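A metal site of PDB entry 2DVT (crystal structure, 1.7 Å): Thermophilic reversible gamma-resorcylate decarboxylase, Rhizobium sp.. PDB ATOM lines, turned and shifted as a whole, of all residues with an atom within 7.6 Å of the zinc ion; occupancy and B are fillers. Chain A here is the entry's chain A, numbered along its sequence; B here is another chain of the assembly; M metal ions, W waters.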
ATOM      1  N   GLU A   8     -23.411  24.293   9.379  1.00  0.00           N
ATOM      2  CA  GLU A   8     -23.767  25.594   9.947  1.00  0.00           C
ATOM      3  C   GLU A   8     -24.047  25.202  11.387  1.00  0.00           C
ATOM      4  O   GLU A   8     -25.192  25.154  11.841  1.00  0.00           O
ATOM      5  CB  GLU A   8     -24.985  26.272   9.320  1.00  0.00           C
ATOM      6  CG  GLU A   8     -25.103  27.708   9.875  1.00  0.00           C
ATOM      7  CD  GLU A   8     -26.229  28.547   9.292  1.00  0.00           C
ATOM      8  OE1 GLU A   8     -26.718  29.430  10.033  1.00  0.00           O
ATOM      9  OE2 GLU A   8     -26.610  28.355   8.130  1.00  0.00           O
ATOM     10  N   GLU A   9     -22.965  24.890  12.081  1.00  0.00           N
ATOM     11  CA  GLU A   9     -22.983  24.415  13.459  1.00  0.00           C
ATOM     12  C   GLU A   9     -22.066  25.346  14.226  1.00  0.00           C
ATOM     13  O   GLU A   9     -20.856  25.368  14.007  1.00  0.00           O
ATOM     14  CB  GLU A   9     -22.466  22.977  13.459  1.00  0.00           C
ATOM     15  CG  GLU A   9     -22.841  22.215  12.176  1.00  0.00           C
ATOM     16  CD  GLU A   9     -24.353  22.042  11.999  1.00  0.00           C
ATOM     17  OE1 GLU A   9     -24.880  22.354  10.909  1.00  0.00           O
ATOM     18  OE2 GLU A   9     -24.998  21.583  12.955  1.00  0.00           O
ATOM     19  N   HIS A  10     -22.655  26.090  15.157  1.00  0.00           N
ATOM     20  CA  HIS A  10     -21.946  27.110  15.904  1.00  0.00           C
ATOM     21  C   HIS A  10     -21.479  26.809  17.321  1.00  0.00           C
ATOM     22  O   HIS A  10     -21.983  25.919  18.000  1.00  0.00           O
ATOM     23  CB  HIS A  10     -22.803  28.374  15.926  1.00  0.00           C
ATOM     24  CG  HIS A  10     -23.330  28.790  14.587  1.00  0.00           C
ATOM     25  ND1 HIS A  10     -22.521  29.291  13.593  1.00  0.00           N
ATOM     26  CD2 HIS A  10     -24.589  28.772  14.078  1.00  0.00           C
ATOM     27  CE1 HIS A  10     -23.257  29.565  12.532  1.00  0.00           C
ATOM     28  NE2 HIS A  10     -24.516  29.265  12.798  1.00  0.00           N
ATOM     29  N   SER A  58     -18.205  26.642  13.343  1.00  0.00           N
ATOM     30  CA  SER A  58     -17.997  28.068  13.098  1.00  0.00           C
ATOM     31  C   SER A  58     -18.415  28.886  14.319  1.00  0.00           C
ATOM     32  O   SER A  58     -19.317  28.507  15.066  1.00  0.00           O
ATOM     33  CB  SER A  58     -18.788  28.525  11.869  1.00  0.00           C
ATOM     34  OG  SER A  58     -20.194  28.398  12.092  1.00  0.00           O
ATOM     35  N   LEU A  59     -17.755  30.028  14.504  1.00  0.00           N
ATOM     36  CA  LEU A  59     -18.032  30.928  15.609  1.00  0.00           C
ATOM     37  C   LEU A  59     -19.458  31.457  15.467  1.00  0.00           C
ATOM     38  O   LEU A  59     -20.020  31.416  14.379  1.00  0.00           O
ATOM     39  CB  LEU A  59     -17.029  32.082  15.581  1.00  0.00           C
ATOM     40  CG  LEU A  59     -17.044  33.114  16.712  1.00  0.00           C
ATOM     41  CD1 LEU A  59     -16.739  32.439  18.054  1.00  0.00           C
ATOM     42  CD2 LEU A  59     -15.999  34.174  16.403  1.00  0.00           C
ATOM     43  N   ASN A  60     -20.039  31.944  16.566  1.00  0.00           N
ATOM     44  CA  ASN A  60     -21.395  32.484  16.525  1.00  0.00           C
ATOM     45  C   ASN A  60     -21.448  33.872  15.884  1.00  0.00           C
ATOM     46  O   ASN A  60     -20.453  34.339  15.342  1.00  0.00           O
ATOM     47  CB  ASN A  60     -22.004  32.486  17.940  1.00  0.00           C
ATOM     48  CG  ASN A  60     -21.224  33.377  18.914  1.00  0.00           C
ATOM     49  OD1 ASN A  60     -19.997  33.427  18.879  1.00  0.00           O
ATOM     50  ND2 ASN A  60     -21.949  34.044  19.799  1.00  0.00           N
ATOM     51  N   ALA A  61     -22.601  34.525  15.946  1.00  0.00           N
ATOM     52  CA  ALA A  61     -22.770  35.822  15.293  1.00  0.00           C
ATOM     53  C   ALA A  61     -23.360  36.919  16.186  1.00  0.00           C
ATOM     54  O   ALA A  61     -24.066  36.643  17.148  1.00  0.00           O
ATOM     55  CB  ALA A  61     -23.643  35.658  14.058  1.00  0.00           C
ATOM     56  N   LEU A 126     -16.423  31.488   7.426  1.00  0.00           N
ATOM     57  CA  LEU A 126     -17.824  31.802   7.689  1.00  0.00           C
ATOM     58  C   LEU A 126     -17.829  33.220   8.236  1.00  0.00           C
ATOM     59  O   LEU A 126     -17.160  33.520   9.240  1.00  0.00           O
ATOM     60  CB  LEU A 126     -18.460  30.830   8.691  1.00  0.00           C
ATOM     61  CG  LEU A 126     -19.961  31.078   8.868  1.00  0.00           C
ATOM     62  CD1 LEU A 126     -20.702  29.767   9.074  1.00  0.00           C
ATOM     63  CD2 LEU A 126     -20.175  32.021  10.035  1.00  0.00           C
ATOM     64  N   ASN A 128     -20.373  36.630   9.157  1.00  0.00           N
ATOM     65  CA  ASN A 128     -21.728  37.083   9.455  1.00  0.00           C
ATOM     66  C   ASN A 128     -22.082  38.407   8.777  1.00  0.00           C
ATOM     67  O   ASN A 128     -22.207  39.440   9.429  1.00  0.00           O
ATOM     68  CB  ASN A 128     -21.899  37.198  10.962  1.00  0.00           C
ATOM     69  CG  ASN A 128     -21.516  35.921  11.678  1.00  0.00           C
ATOM     70  OD1 ASN A 128     -22.043  34.849  11.374  1.00  0.00           O
ATOM     71  ND2 ASN A 128     -20.579  36.016  12.625  1.00  0.00           N
ATOM     72  N   TYR A 162     -18.769  30.937   3.507  1.00  0.00           N
ATOM     73  CA  TYR A 162     -20.150  30.835   3.981  1.00  0.00           C
ATOM     74  C   TYR A 162     -20.618  32.224   4.406  1.00  0.00           C
ATOM     75  O   TYR A 162     -20.142  32.767   5.406  1.00  0.00           O
ATOM     76  CB  TYR A 162     -20.217  29.861   5.173  1.00  0.00           C
ATOM     77  CG  TYR A 162     -21.577  29.240   5.431  1.00  0.00           C
ATOM     78  CD1 TYR A 162     -21.730  27.848   5.491  1.00  0.00           C
ATOM     79  CD2 TYR A 162     -22.706  30.031   5.639  1.00  0.00           C
ATOM     80  CE1 TYR A 162     -22.962  27.261   5.763  1.00  0.00           C
ATOM     81  CE2 TYR A 162     -23.953  29.453   5.908  1.00  0.00           C
ATOM     82  CZ  TYR A 162     -24.075  28.068   5.974  1.00  0.00           C
ATOM     83  OH  TYR A 162     -25.286  27.483   6.252  1.00  0.00           O
ATOM     84  N   HIS A 164     -23.015  34.079   6.168  1.00  0.00           N
ATOM     85  CA  HIS A 164     -23.991  33.888   7.243  1.00  0.00           C
ATOM     86  C   HIS A 164     -24.709  35.206   7.589  1.00  0.00           C
ATOM     87  O   HIS A 164     -24.199  36.290   7.311  1.00  0.00           O
ATOM     88  CB  HIS A 164     -23.248  33.332   8.470  1.00  0.00           C
ATOM     89  CG  HIS A 164     -24.132  32.857   9.580  1.00  0.00           C
ATOM     90  ND1 HIS A 164     -24.638  33.703  10.551  1.00  0.00           N
ATOM     91  CD2 HIS A 164     -24.590  31.619   9.880  1.00  0.00           C
ATOM     92  CE1 HIS A 164     -25.363  33.005  11.395  1.00  0.00           C
ATOM     93  NE2 HIS A 164     -25.358  31.738  11.019  1.00  0.00           N
ATOM     94  N   PRO A 165     -25.908  35.113   8.187  1.00  0.00           N
ATOM     95  CA  PRO A 165     -26.656  36.317   8.542  1.00  0.00           C
ATOM     96  C   PRO A 165     -26.161  37.137   9.738  1.00  0.00           C
ATOM     97  O   PRO A 165     -25.349  36.689  10.547  1.00  0.00           O
ATOM     98  CB  PRO A 165     -28.064  35.797   8.830  1.00  0.00           C
ATOM     99  CG  PRO A 165     -28.133  34.515   8.061  1.00  0.00           C
ATOM    100  CD  PRO A 165     -26.772  33.925   8.285  1.00  0.00           C
ATOM    101  N   PHE A 189     -32.730  38.472   9.128  1.00  0.00           N
ATOM    102  CA  PHE A 189     -31.532  37.713   8.765  1.00  0.00           C
ATOM    103  C   PHE A 189     -31.523  37.352   7.273  1.00  0.00           C
ATOM    104  O   PHE A 189     -30.503  37.499   6.592  1.00  0.00           O
ATOM    105  CB  PHE A 189     -31.452  36.405   9.567  1.00  0.00           C
ATOM    106  CG  PHE A 189     -30.769  36.528  10.906  1.00  0.00           C
ATOM    107  CD1 PHE A 189     -30.600  35.407  11.709  1.00  0.00           C
ATOM    108  CD2 PHE A 189     -30.289  37.759  11.365  1.00  0.00           C
ATOM    109  CE1 PHE A 189     -29.961  35.507  12.944  1.00  0.00           C
ATOM    110  CE2 PHE A 189     -29.652  37.863  12.591  1.00  0.00           C
ATOM    111  CZ  PHE A 189     -29.490  36.730  13.390  1.00  0.00           C
ATOM    112  N   GLY A 217     -27.088  29.726   4.092  1.00  0.00           N
ATOM    113  CA  GLY A 217     -27.886  28.817   4.884  1.00  0.00           C
ATOM    114  C   GLY A 217     -29.370  29.129   4.728  1.00  0.00           C
ATOM    115  O   GLY A 217     -29.760  29.919   3.867  1.00  0.00           O
ATOM    116  N   HIS A 218     -30.189  28.474   5.552  1.00  0.00           N
ATOM    117  CA  HIS A 218     -31.631  28.722   5.561  1.00  0.00           C
ATOM    118  C   HIS A 218     -32.266  28.631   4.177  1.00  0.00           C
ATOM    119  O   HIS A 218     -33.147  29.422   3.823  1.00  0.00           O
ATOM    120  CB  HIS A 218     -31.865  30.085   6.194  1.00  0.00           C
ATOM    121  CG  HIS A 218     -30.949  30.343   7.359  1.00  0.00           C
ATOM    122  ND1 HIS A 218     -29.830  31.153   7.260  1.00  0.00           N
ATOM    123  CD2 HIS A 218     -30.889  29.770   8.582  1.00  0.00           C
ATOM    124  CE1 HIS A 218     -29.134  31.076   8.375  1.00  0.00           C
ATOM    125  NE2 HIS A 218     -29.751  30.234   9.194  1.00  0.00           N
ATOM    126  N   SER A 262     -30.085  24.587   6.913  1.00  0.00           N
ATOM    127  CA  SER A 262     -30.054  25.116   8.271  1.00  0.00           C
ATOM    128  C   SER A 262     -31.305  25.902   8.640  1.00  0.00           C
ATOM    129  O   SER A 262     -31.742  26.789   7.913  1.00  0.00           O
ATOM    130  CB  SER A 262     -28.816  25.998   8.475  1.00  0.00           C
ATOM    131  OG  SER A 262     -28.873  27.169   7.689  1.00  0.00           O
ATOM    132  N   GLY A 263     -31.890  25.553   9.786  1.00  0.00           N
ATOM    133  CA  GLY A 263     -33.083  26.243  10.263  1.00  0.00           C
ATOM    134  C   GLY A 263     -34.241  26.406   9.294  1.00  0.00           C
ATOM    135  O   GLY A 263     -35.038  27.325   9.434  1.00  0.00           O
ATOM    136  N   THR A 286     -27.810  22.089  10.279  1.00  0.00           N
ATOM    137  CA  THR A 286     -28.836  22.237  11.311  1.00  0.00           C
ATOM    138  C   THR A 286     -29.027  23.605  11.958  1.00  0.00           C
ATOM    139  O   THR A 286     -30.157  23.985  12.280  1.00  0.00           O
ATOM    140  CB  THR A 286     -28.586  21.238  12.456  1.00  0.00           C
ATOM    141  OG1 THR A 286     -27.478  21.687  13.255  1.00  0.00           O
ATOM    142  CG2 THR A 286     -28.250  19.852  11.896  1.00  0.00           C
ATOM    143  N   ASP A 287     -27.933  24.327  12.146  1.00  0.00           N
ATOM    144  CA  ASP A 287     -27.905  25.631  12.799  1.00  0.00           C
ATOM    145  C   ASP A 287     -27.866  25.432  14.314  1.00  0.00           C
ATOM    146  O   ASP A 287     -28.288  26.290  15.092  1.00  0.00           O
ATOM    147  CB  ASP A 287     -29.113  26.506  12.410  1.00  0.00           C
ATOM    148  CG  ASP A 287     -28.766  27.982  12.359  1.00  0.00           C
ATOM    149  OD1 ASP A 287     -27.627  28.337  12.752  1.00  0.00           O
ATOM    150  OD2 ASP A 287     -29.617  28.790  11.935  1.00  0.00           O
ATOM    151  N   TRP A 288     -27.363  24.270  14.729  1.00  0.00           N
ATOM    152  CA  TRP A 288     -27.200  23.977  16.147  1.00  0.00           C
ATOM    153  C   TRP A 288     -26.227  25.055  16.625  1.00  0.00           C
ATOM    154  O   TRP A 288     -25.339  25.464  15.862  1.00  0.00           O
ATOM    155  CB  TRP A 288     -26.595  22.575  16.315  1.00  0.00           C
ATOM    156  CG  TRP A 288     -26.124  22.262  17.713  1.00  0.00           C
ATOM    157  CD1 TRP A 288     -24.860  22.375  18.211  1.00  0.00           C
ATOM    158  CD2 TRP A 288     -26.941  21.776  18.798  1.00  0.00           C
ATOM    159  NE1 TRP A 288     -24.825  22.001  19.532  1.00  0.00           N
ATOM    160  CE2 TRP A 288     -26.085  21.625  19.921  1.00  0.00           C
ATOM    161  CE3 TRP A 288     -28.293  21.461  18.920  1.00  0.00           C
ATOM    162  CZ2 TRP A 288     -26.566  21.171  21.156  1.00  0.00           C
ATOM    163  CZ3 TRP A 288     -28.765  21.010  20.154  1.00  0.00           C
ATOM    164  CH2 TRP A 288     -27.893  20.867  21.253  1.00  0.00           C
ATOM    165  N   PRO A 289     -26.354  25.522  17.881  1.00  0.00           N
ATOM    166  CA  PRO A 289     -27.324  25.139  18.914  1.00  0.00           C
ATOM    167  C   PRO A 289     -28.615  25.961  18.906  1.00  0.00           C
ATOM    168  O   PRO A 289     -29.435  25.827  19.813  1.00  0.00           O
ATOM    169  CB  PRO A 289     -26.529  25.347  20.194  1.00  0.00           C
ATOM    170  CG  PRO A 289     -25.788  26.604  19.878  1.00  0.00           C
ATOM    171  CD  PRO A 289     -25.321  26.410  18.440  1.00  0.00           C
ATOM    172  N   PHE A 290     -28.789  26.796  17.888  1.00  0.00           N
ATOM    173  CA  PHE A 290     -29.993  27.620  17.785  1.00  0.00           C
ATOM    174  C   PHE A 290     -31.192  26.774  17.344  1.00  0.00           C
ATOM    175  O   PHE A 290     -32.346  27.158  17.546  1.00  0.00           O
ATOM    176  CB  PHE A 290     -29.726  28.770  16.810  1.00  0.00           C
ATOM    177  CG  PHE A 290     -28.567  29.631  17.225  1.00  0.00           C
ATOM    178  CD1 PHE A 290     -28.688  30.510  18.309  1.00  0.00           C
ATOM    179  CD2 PHE A 290     -27.340  29.532  16.578  1.00  0.00           C
ATOM    180  CE1 PHE A 290     -27.605  31.264  18.737  1.00  0.00           C
ATOM    181  CE2 PHE A 290     -26.236  30.289  17.013  1.00  0.00           C
ATOM    182  CZ  PHE A 290     -26.375  31.157  18.085  1.00  0.00           C
ATOM    183  N   ARG B 229     -40.253  28.830   8.243  1.00  0.00           N
ATOM    184  CA  ARG B 229     -39.182  29.383   9.072  1.00  0.00           C
ATOM    185  C   ARG B 229     -39.624  30.605   9.881  1.00  0.00           C
ATOM    186  O   ARG B 229     -39.212  30.768  11.029  1.00  0.00           O
ATOM    187  CB  ARG B 229     -37.975  29.749   8.193  1.00  0.00           C
ATOM    188  CG  ARG B 229     -36.781  30.329   8.965  1.00  0.00           C
ATOM    189  CD  ARG B 229     -35.552  30.383   8.070  1.00  0.00           C
ATOM    190  NE  ARG B 229     -34.501  31.246   8.600  1.00  0.00           N
ATOM    191  CZ  ARG B 229     -33.742  30.967   9.662  1.00  0.00           C
ATOM    192  NH1 ARG B 229     -33.917  29.840  10.331  1.00  0.00           N
ATOM    193  NH2 ARG B 229     -32.802  31.828  10.037  1.00  0.00           N
HETATM  194 ZN    ZN M   1     -26.327  30.071  11.900  1.00  0.00          ZN
HETATM  195  O   HOH W   1     -27.191  31.278  13.420  1.00  0.00           O
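NE2 of His 218 sits close to OE1 of Glu 8, 3.2 Å away. The side-chain carboxylate of Glu 8 sits at hydrogen-bond distance from the side-chain hydroxyl of Ser 262. OE2 of Glu 8 is in hydrogen-bond range of OH of Tyr 162 (2.5 Å). The side-chain amide oxygen (OD1) of Asn 128 sits at hydrogen-bond distance from a ring nitrogen (ND1) of His 164 (3.0 Å). The backbone carbonyl oxygen (O) of Trp 288 is in hydrogen-bond range of the backbone NH (N) of His 10 (2.8 Å). A ring nitrogen (ND1) of His 10 sits at hydrogen-bond distance from the side-chain hydroxyl (OG) of Ser 58 (2.9 Å). A ring nitrogen (ND1) of His 10 lies within hydrogen-bond range of the backbone carbonyl oxygen of Leu 59 (3.4 Å). The side-chain carboxylate (OD2) of Asp 287 sits at hydrogen-bond distance from a ring nitrogen (NE2) of His 218 (3.1 Å).
Four residues have an atom within 4 Å of the zinc ion: Glu 8, His 10, His 164 and Asp 287. Along chain A the residues within 4 Å of the zinc ion span positions 8 to 287. The nearest printed residue that does not touch the zinc ion is His 218 (4.4 Å).
OE1 of Glu 8 binds the zinc ion (2.0 Å). The zinc ion is bound by NE2 of His 164 (2.1 Å). Water W1 is bound to the zinc ion, 2.1 Å away. The zinc ion is bound by NE2 of His 10, 2.2 Å away. The zinc ion is bound by OD1 of Asp 287.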
